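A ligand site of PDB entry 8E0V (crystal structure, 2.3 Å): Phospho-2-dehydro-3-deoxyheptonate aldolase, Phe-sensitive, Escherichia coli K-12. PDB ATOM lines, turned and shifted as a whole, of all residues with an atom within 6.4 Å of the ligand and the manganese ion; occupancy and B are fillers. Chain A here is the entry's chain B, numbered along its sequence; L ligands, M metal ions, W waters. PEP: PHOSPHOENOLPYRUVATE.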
ATOM      1  N   CYS A  62       3.491  17.256  19.811  1.00  0.00           N
ATOM      2  CA  CYS A  62       3.921  17.529  18.448  1.00  0.00           C
ATOM      3  C   CYS A  62       3.912  16.251  17.628  1.00  0.00           C
ATOM      4  O   CYS A  62       3.406  16.225  16.495  1.00  0.00           O
ATOM      5  CB  CYS A  62       5.310  18.157  18.446  1.00  0.00           C
ATOM      6  SG  CYS A  62       6.055  18.316  16.812  1.00  0.00           S
ATOM      7  N   SER A  63       4.473  15.176  18.190  1.00  0.00           N
ATOM      8  CA  SER A  63       4.563  13.876  17.525  1.00  0.00           C
ATOM      9  C   SER A  63       4.401  12.809  18.581  1.00  0.00           C
ATOM     10  O   SER A  63       4.866  12.985  19.708  1.00  0.00           O
ATOM     11  CB  SER A  63       5.905  13.684  16.813  1.00  0.00           C
ATOM     12  OG  SER A  63       6.962  13.576  17.752  1.00  0.00           O
ATOM     13  N   ARG A  93      -4.154  15.822  19.784  1.00  0.00           N
ATOM     14  CA  ARG A  93      -3.162  15.604  18.731  1.00  0.00           C
ATOM     15  C   ARG A  93      -2.576  14.196  18.817  1.00  0.00           C
ATOM     16  O   ARG A  93      -1.916  13.825  19.794  1.00  0.00           O
ATOM     17  CB  ARG A  93      -2.041  16.639  18.831  1.00  0.00           C
ATOM     18  CG  ARG A  93      -2.455  18.033  18.415  1.00  0.00           C
ATOM     19  CD  ARG A  93      -1.247  18.990  18.449  1.00  0.00           C
ATOM     20  NE  ARG A  93      -0.072  18.447  17.752  1.00  0.00           N
ATOM     21  CZ  ARG A  93       0.421  18.936  16.628  1.00  0.00           C
ATOM     22  NH1 ARG A  93      -0.164  19.953  15.996  1.00  0.00           N
ATOM     23  NH2 ARG A  93       1.536  18.410  16.115  1.00  0.00           N
ATOM     24  N   TYR A  95      -0.323  12.767  16.230  1.00  0.00           N
ATOM     25  CA  TYR A  95       0.342  12.921  14.941  1.00  0.00           C
ATOM     26  C   TYR A  95       1.349  11.799  14.726  1.00  0.00           C
ATOM     27  O   TYR A  95       2.315  11.684  15.480  1.00  0.00           O
ATOM     28  CB  TYR A  95       1.019  14.296  14.842  1.00  0.00           C
ATOM     29  CG  TYR A  95       0.061  15.446  14.524  1.00  0.00           C
ATOM     30  CD1 TYR A  95      -1.219  15.490  15.080  1.00  0.00           C
ATOM     31  CD2 TYR A  95       0.457  16.480  13.705  1.00  0.00           C
ATOM     32  CE1 TYR A  95      -2.105  16.529  14.786  1.00  0.00           C
ATOM     33  CE2 TYR A  95      -0.407  17.550  13.430  1.00  0.00           C
ATOM     34  CZ  TYR A  95      -1.678  17.564  13.965  1.00  0.00           C
ATOM     35  OH  TYR A  95      -2.524  18.614  13.669  1.00  0.00           O
ATOM     36  N   GLU A  97       2.810  11.415  11.560  1.00  0.00           N
ATOM     37  CA  GLU A  97       3.560  11.788  10.370  1.00  0.00           C
ATOM     38  C   GLU A  97       4.080  13.208  10.521  1.00  0.00           C
ATOM     39  O   GLU A  97       3.313  14.119  10.869  1.00  0.00           O
ATOM     40  CB  GLU A  97       2.697  11.672   9.116  1.00  0.00           C
ATOM     41  CG  GLU A  97       1.781  10.447   9.081  1.00  0.00           C
ATOM     42  CD  GLU A  97       1.230  10.135   7.656  1.00  0.00           C
ATOM     43  OE1 GLU A  97       0.732  11.063   6.947  1.00  0.00           O
ATOM     44  OE2 GLU A  97       1.314   8.931   7.243  1.00  0.00           O
ATOM     45  N   LYS A  98       5.370  13.379  10.318  1.00  0.00           N
ATOM     46  CA  LYS A  98       5.985  14.699  10.542  1.00  0.00           C
ATOM     47  C   LYS A  98       6.679  15.162   9.266  1.00  0.00           C
ATOM     48  O   LYS A  98       7.514  14.425   8.726  1.00  0.00           O
ATOM     49  CB  LYS A  98       6.927  14.617  11.738  1.00  0.00           C
ATOM     50  CG  LYS A  98       6.313  14.064  13.018  1.00  0.00           C
ATOM     51  CD  LYS A  98       5.146  14.890  13.529  1.00  0.00           C
ATOM     52  CE  LYS A  98       5.438  16.371  13.564  1.00  0.00           C
ATOM     53  NZ  LYS A  98       4.269  17.147  14.034  1.00  0.00           N
ATOM     54  N   PRO A  99       6.351  16.359   8.742  1.00  0.00           N
ATOM     55  CA  PRO A  99       7.071  16.900   7.576  1.00  0.00           C
ATOM     56  C   PRO A  99       8.346  17.591   8.053  1.00  0.00           C
ATOM     57  O   PRO A  99       8.305  18.376   8.998  1.00  0.00           O
ATOM     58  CB  PRO A  99       6.078  17.904   6.977  1.00  0.00           C
ATOM     59  CG  PRO A  99       5.304  18.411   8.202  1.00  0.00           C
ATOM     60  CD  PRO A  99       5.269  17.246   9.198  1.00  0.00           C
ATOM     61  N   GLU A 144      -2.248  15.031  11.286  1.00  0.00           N
ATOM     62  CA  GLU A 144      -1.896  15.622  10.002  1.00  0.00           C
ATOM     63  C   GLU A 144      -1.870  14.529   8.933  1.00  0.00           C
ATOM     64  O   GLU A 144      -1.232  13.479   9.111  1.00  0.00           O
ATOM     65  CB  GLU A 144      -0.537  16.350  10.024  1.00  0.00           C
ATOM     66  CG  GLU A 144      -0.260  17.102   8.666  1.00  0.00           C
ATOM     67  CD  GLU A 144       1.159  17.693   8.502  1.00  0.00           C
ATOM     68  OE1 GLU A 144       1.818  17.961   9.530  1.00  0.00           O
ATOM     69  OE2 GLU A 144       1.610  17.913   7.317  1.00  0.00           O
ATOM     70  N   ALA A 162      -5.430  17.759   9.578  1.00  0.00           N
ATOM     71  CA  ALA A 162      -4.752  18.969   9.146  1.00  0.00           C
ATOM     72  C   ALA A 162      -3.942  18.683   7.892  1.00  0.00           C
ATOM     73  O   ALA A 162      -3.321  17.618   7.770  1.00  0.00           O
ATOM     74  CB  ALA A 162      -3.841  19.528  10.243  1.00  0.00           C
ATOM     75  N   ILE A 163      -3.972  19.627   6.956  1.00  0.00           N
ATOM     76  CA  ILE A 163      -2.962  19.699   5.907  1.00  0.00           C
ATOM     77  C   ILE A 163      -1.931  20.728   6.343  1.00  0.00           C
ATOM     78  O   ILE A 163      -2.281  21.871   6.660  1.00  0.00           O
ATOM     79  CB  ILE A 163      -3.574  20.036   4.545  1.00  0.00           C
ATOM     80  CG1 ILE A 163      -4.687  19.044   4.244  1.00  0.00           C
ATOM     81  CG2 ILE A 163      -2.483  19.958   3.488  1.00  0.00           C
ATOM     82  CD1 ILE A 163      -4.238  17.576   4.216  1.00  0.00           C
ATOM     83  N   GLY A 164      -0.662  20.294   6.423  1.00  0.00           N
ATOM     84  CA  GLY A 164       0.368  21.131   7.006  1.00  0.00           C
ATOM     85  C   GLY A 164       0.592  22.375   6.170  1.00  0.00           C
ATOM     86  O   GLY A 164       0.085  22.499   5.049  1.00  0.00           O
ATOM     87  N   ALA A 165       1.340  23.321   6.741  1.00  0.00           N
ATOM     88  CA  ALA A 165       1.702  24.544   6.037  1.00  0.00           C
ATOM     89  C   ALA A 165       2.452  24.207   4.766  1.00  0.00           C
ATOM     90  O   ALA A 165       2.308  24.902   3.743  1.00  0.00           O
ATOM     91  CB  ALA A 165       2.590  25.415   6.940  1.00  0.00           C
ATOM     92  N   ARG A 166       3.282  23.161   4.803  1.00  0.00           N
ATOM     93  CA  ARG A 166       4.180  22.893   3.665  1.00  0.00           C
ATOM     94  C   ARG A 166       3.500  22.096   2.561  1.00  0.00           C
ATOM     95  O   ARG A 166       4.143  21.835   1.538  1.00  0.00           O
ATOM     96  CB  ARG A 166       5.452  22.154   4.111  1.00  0.00           C
ATOM     97  CG  ARG A 166       6.392  22.946   5.030  1.00  0.00           C
ATOM     98  CD  ARG A 166       7.232  21.997   5.928  1.00  0.00           C
ATOM     99  NE  ARG A 166       7.920  22.725   6.991  1.00  0.00           N
ATOM    100  CZ  ARG A 166       7.365  23.014   8.170  1.00  0.00           C
ATOM    101  NH1 ARG A 166       6.145  22.602   8.495  1.00  0.00           N
ATOM    102  NH2 ARG A 166       8.042  23.755   9.033  1.00  0.00           N
ATOM    103  N   LYS A 187      -3.134  24.680   7.122  1.00  0.00           N
ATOM    104  CA  LYS A 187      -2.269  25.717   7.658  1.00  0.00           C
ATOM    105  C   LYS A 187      -2.037  26.794   6.598  1.00  0.00           C
ATOM    106  O   LYS A 187      -2.105  26.532   5.396  1.00  0.00           O
ATOM    107  CB  LYS A 187      -0.927  25.148   8.102  1.00  0.00           C
ATOM    108  CG  LYS A 187      -1.038  24.051   9.165  1.00  0.00           C
ATOM    109  CD  LYS A 187      -1.425  24.619  10.508  1.00  0.00           C
ATOM    110  CE  LYS A 187      -1.061  23.673  11.665  1.00  0.00           C
ATOM    111  NZ  LYS A 187       0.342  23.843  12.207  1.00  0.00           N
ATOM    112  N   ASN A 188      -1.684  27.969   7.106  1.00  0.00           N
ATOM    113  CA  ASN A 188      -1.274  29.055   6.186  1.00  0.00           C
ATOM    114  C   ASN A 188       0.146  28.730   5.768  1.00  0.00           C
ATOM    115  O   ASN A 188       0.759  27.854   6.391  1.00  0.00           O
ATOM    116  CB  ASN A 188      -1.417  30.445   6.816  1.00  0.00           C
ATOM    117  CG  ASN A 188      -0.556  30.672   8.042  1.00  0.00           C
ATOM    118  OD1 ASN A 188      -1.064  30.772   9.145  1.00  0.00           O
ATOM    119  ND2 ASN A 188       0.744  30.812   7.838  1.00  0.00           N
ATOM    120  N   THR A 190       4.260  28.924   5.051  1.00  0.00           N
ATOM    121  CA  THR A 190       5.404  29.107   5.969  1.00  0.00           C
ATOM    122  C   THR A 190       5.808  30.588   6.017  1.00  0.00           C
ATOM    123  O   THR A 190       6.326  30.996   7.055  1.00  0.00           O
ATOM    124  CB  THR A 190       6.547  28.170   5.528  1.00  0.00           C
ATOM    125  OG1 THR A 190       6.775  28.322   4.135  1.00  0.00           O
ATOM    126  CG2 THR A 190       6.234  26.723   5.836  1.00  0.00           C
ATOM    127  N   ARG A 235      -0.918  29.994  11.740  1.00  0.00           N
ATOM    128  CA  ARG A 235       0.198  29.320  12.416  1.00  0.00           C
ATOM    129  C   ARG A 235       1.459  30.179  12.315  1.00  0.00           C
ATOM    130  O   ARG A 235       2.517  29.709  12.718  1.00  0.00           O
ATOM    131  CB  ARG A 235       0.399  27.951  11.753  1.00  0.00           C
ATOM    132  CG  ARG A 235       0.370  27.984  10.233  1.00  0.00           C
ATOM    133  CD  ARG A 235       1.737  28.270   9.656  1.00  0.00           C
ATOM    134  NE  ARG A 235       2.765  27.378  10.174  1.00  0.00           N
ATOM    135  CZ  ARG A 235       4.061  27.627  10.103  1.00  0.00           C
ATOM    136  NH1 ARG A 235       4.492  28.738   9.543  1.00  0.00           N
ATOM    137  NH2 ARG A 235       4.927  26.754  10.591  1.00  0.00           N
ATOM    138  N   ASP A 266      -3.355  28.321  15.643  1.00  0.00           N
ATOM    139  CA  ASP A 266      -2.317  27.449  16.161  1.00  0.00           C
ATOM    140  C   ASP A 266      -1.419  28.291  17.063  1.00  0.00           C
ATOM    141  O   ASP A 266      -0.841  29.291  16.604  1.00  0.00           O
ATOM    142  CB  ASP A 266      -1.509  26.851  15.004  1.00  0.00           C
ATOM    143  CG  ASP A 266      -0.315  26.041  15.463  1.00  0.00           C
ATOM    144  OD1 ASP A 266      -0.282  25.663  16.668  1.00  0.00           O
ATOM    145  OD2 ASP A 266       0.570  25.748  14.626  1.00  0.00           O
ATOM    146  N   SER A 268       1.371  27.346  18.430  1.00  0.00           N
ATOM    147  CA  SER A 268       2.756  26.884  18.413  1.00  0.00           C
ATOM    148  C   SER A 268       3.428  27.278  17.087  1.00  0.00           C
ATOM    149  O   SER A 268       2.992  28.206  16.415  1.00  0.00           O
ATOM    150  CB  SER A 268       2.760  25.370  18.651  1.00  0.00           C
ATOM    151  OG  SER A 268       4.093  24.896  18.786  1.00  0.00           O
ATOM    152  N   HIS A 269       4.513  26.579  16.733  1.00  0.00           N
ATOM    153  CA  HIS A 269       5.291  26.782  15.489  1.00  0.00           C
ATOM    154  C   HIS A 269       5.655  28.256  15.369  1.00  0.00           C
ATOM    155  O   HIS A 269       6.188  28.825  16.328  1.00  0.00           O
ATOM    156  CB  HIS A 269       4.508  26.185  14.343  1.00  0.00           C
ATOM    157  CG  HIS A 269       4.042  24.788  14.620  1.00  0.00           C
ATOM    158  ND1 HIS A 269       2.754  24.485  15.011  1.00  0.00           N
ATOM    159  CD2 HIS A 269       4.722  23.611  14.644  1.00  0.00           C
ATOM    160  CE1 HIS A 269       2.646  23.191  15.239  1.00  0.00           C
ATOM    161  NE2 HIS A 269       3.828  22.641  15.012  1.00  0.00           N
ATOM    162  N   MET A 301      -5.082  25.308  18.495  1.00  0.00           N
ATOM    163  CA  MET A 301      -4.232  24.132  18.518  1.00  0.00           C
ATOM    164  C   MET A 301      -3.023  24.466  19.364  1.00  0.00           C
ATOM    165  O   MET A 301      -2.531  25.600  19.342  1.00  0.00           O
ATOM    166  CB  MET A 301      -3.872  23.706  17.078  1.00  0.00           C
ATOM    167  CG  MET A 301      -2.520  23.047  16.830  1.00  0.00           C
ATOM    168  SD  MET A 301      -2.130  22.676  15.048  1.00  0.00           S
ATOM    169  CE  MET A 301      -3.571  21.797  14.458  1.00  0.00           C
ATOM    170  N   GLU A 303       0.664  22.579  21.226  1.00  0.00           N
ATOM    171  CA  GLU A 303       1.598  21.473  21.316  1.00  0.00           C
ATOM    172  C   GLU A 303       1.945  21.243  22.785  1.00  0.00           C
ATOM    173  O   GLU A 303       2.697  22.018  23.393  1.00  0.00           O
ATOM    174  CB  GLU A 303       2.817  21.743  20.437  1.00  0.00           C
ATOM    175  CG  GLU A 303       2.490  21.514  18.910  1.00  0.00           C
ATOM    176  CD  GLU A 303       3.721  21.524  18.037  1.00  0.00           C
ATOM    177  OE1 GLU A 303       4.620  22.386  18.268  1.00  0.00           O
ATOM    178  OE2 GLU A 303       3.782  20.699  17.090  1.00  0.00           O
ATOM    179  N   THR A 326      10.361  16.011  18.762  1.00  0.00           N
ATOM    180  CA  THR A 326      10.320  16.957  17.656  1.00  0.00           C
ATOM    181  C   THR A 326      10.267  18.358  18.281  1.00  0.00           C
ATOM    182  O   THR A 326      11.197  18.732  18.984  1.00  0.00           O
ATOM    183  CB  THR A 326       9.195  16.605  16.695  1.00  0.00           C
ATOM    184  OG1 THR A 326       7.987  16.367  17.423  1.00  0.00           O
ATOM    185  CG2 THR A 326       9.558  15.329  15.903  1.00  0.00           C
ATOM    186  N   ASP A 327       9.215  19.146  18.023  1.00  0.00           N
ATOM    187  CA  ASP A 327       9.196  20.518  18.535  1.00  0.00           C
ATOM    188  C   ASP A 327       9.003  20.524  20.049  1.00  0.00           C
ATOM    189  O   ASP A 327       8.523  19.563  20.634  1.00  0.00           O
ATOM    190  CB  ASP A 327       8.081  21.341  17.891  1.00  0.00           C
ATOM    191  CG  ASP A 327       8.193  21.415  16.383  1.00  0.00           C
ATOM    192  OD1 ASP A 327       9.336  21.329  15.864  1.00  0.00           O
ATOM    193  OD2 ASP A 327       7.142  21.579  15.715  1.00  0.00           O
HETATM  194  C1  PEP L   1       2.060  20.631  12.971  1.00  0.00           C
HETATM  195  O1  PEP L   1       1.087  21.270  13.358  1.00  0.00           O
HETATM  196  O2' PEP L   1       2.331  19.496  13.370  1.00  0.00           O
HETATM  197  C2  PEP L   1       2.870  21.211  11.971  1.00  0.00           C
HETATM  198  C3  PEP L   1       3.894  20.587  11.251  1.00  0.00           C
HETATM  199  O2  PEP L   1       2.615  22.524  11.695  1.00  0.00           O
HETATM  200  P   PEP L   1       3.003  23.306  10.361  1.00  0.00           P
HETATM  201  O1P PEP L   1       2.600  22.471   9.190  1.00  0.00           O
HETATM  202  O2P PEP L   1       2.245  24.591  10.394  1.00  0.00           O
HETATM  203  O3P PEP L   1       4.474  23.544  10.369  1.00  0.00           O
HETATM  204 MN    MN M   1       5.192  20.706  15.846  1.00  0.00          MN
HETATM  205  O   HOH W   1       4.091  21.460   7.155  1.00  0.00           O
HETATM  206  O   HOH W   2      -1.395  20.394  12.097  1.00  0.00           O
HETATM  207  O   HOH W   3       2.950  17.158  11.506  1.00  0.00           O
HETATM  208  O   HOH W   4       6.899  20.855  13.184  1.00  0.00           O
HETATM  209  O   HOH W   5       6.702  23.558  11.642  1.00  0.00           O
HETATM  210  O   HOH W   6       0.471  20.645  10.099  1.00  0.00           O
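NE2 of His 269 lies close to O1 of the ligand (3.5 Å).
An oxygen (O2P) of the ligand is in salt-bridge range of the side-chain amino group (NZ) of Lys 187 (2.7 Å).
O3P of the ligand lies within salt-bridge range of NH1 of Arg 166.
The guanidinium group (NE) of Arg 235 lies within salt-bridge range of an oxygen (O2P) of the ligand (2.8 Å).
An oxygen (O1P) of the ligand lies within hydrogen-bond range of the backbone NH (N) of Ala 165, 2.9 Å away.
The guanidinium group (NH2) of Arg 93 is in salt-bridge range of an oxygen (O2') of the ligand (3.1 Å).
The side-chain amino group (NZ) of Lys 98 lies within salt-bridge range of an oxygen (O2') of the ligand (3.1 Å).
OG of Ser 268 sits at hydrogen-bond distance from OE1 of Glu 303 (2.6 Å).
The side-chain carboxylate of Asp 266 is in hydrogen-bond range of a ring nitrogen (ND1) of His 269 (2.6 Å).
The side-chain carboxylate (OD2) of Asp 266 lies within salt-bridge range of the side-chain amino group (NZ) of Lys 187, 3.1 Å away.
O of Ile 163 is in hydrogen-bond range of N of Lys 187 (3.0 Å).
O of Cys 62 sits at hydrogen-bond distance from NH2 of Arg 93 (2.9 Å).
The backbone carbonyl oxygen (O) of Cys 62 sits at hydrogen-bond distance from the side-chain amino group (NZ) of Lys 98 (2.8 Å).
SG of Cys 62 sits close to OG1 of Thr 326, at 2.8 Å.
The side-chain carboxylate of Glu 144 lies within hydrogen-bond range of the backbone NH of Gly 164.
Merely in contact with the ligand: Tyr 95, Gly 164, Glu 144 and Met 301.
Hydrophobic or aromatic side chains that line the ligand: Tyr 95, Ala 165, His 269 and Met 301.
11 residues have an atom within 4 Å of the ligand: Arg 93, Tyr 95, Lys 98, Glu 144, Gly 164, Ala 165, Arg 166, Lys 187, Arg 235, His 269 and Met 301.
Four residues have an atom within 4 Å of the manganese ion: Cys 62, His 269, Glu 303 and Asp 327.
The nearest printed residue that does not touch the manganese ion is Lys 98 (4.1 Å).
The manganese ion is bound by OE2 of Glu 303, 1.9 Å away.
OD2 of Asp 327 is bound to the manganese ion.
The manganese ion is bound by NE2 of His 269, 2.5 Å away.
The manganese ion is bound by SG of Cys 62, at 2.7 Å.
The manganese ion has four donor atoms within binding distance.
Water W5 lies within hydrogen-bond range of an oxygen (O3P) of the ligand and the guanidinium group (NH2) of Arg 166.
Water W1 lies within hydrogen-bond range of the guanidinium group of Arg 166 (2.7 Å), an oxygen (O1P) of the ligand (2.7 Å) and the backbone NH of Ala 165 (3.3 Å).
Water W2 lies within hydrogen-bond range of OH of Tyr 95 (2.6 Å) and O1 of the ligand (2.9 Å).
Water W6 bridges an oxygen (O1P) of the ligand (2.9 Å) and the side-chain carboxylate of Glu 144 (3.1 Å).
Water W3 lies within hydrogen-bond range of OE1 of Glu 144 (2.4 Å), NZ of Lys 98 (2.9 Å), O2' of the ligand (3.1 Å) and O of Glu 97 (3.1 Å).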
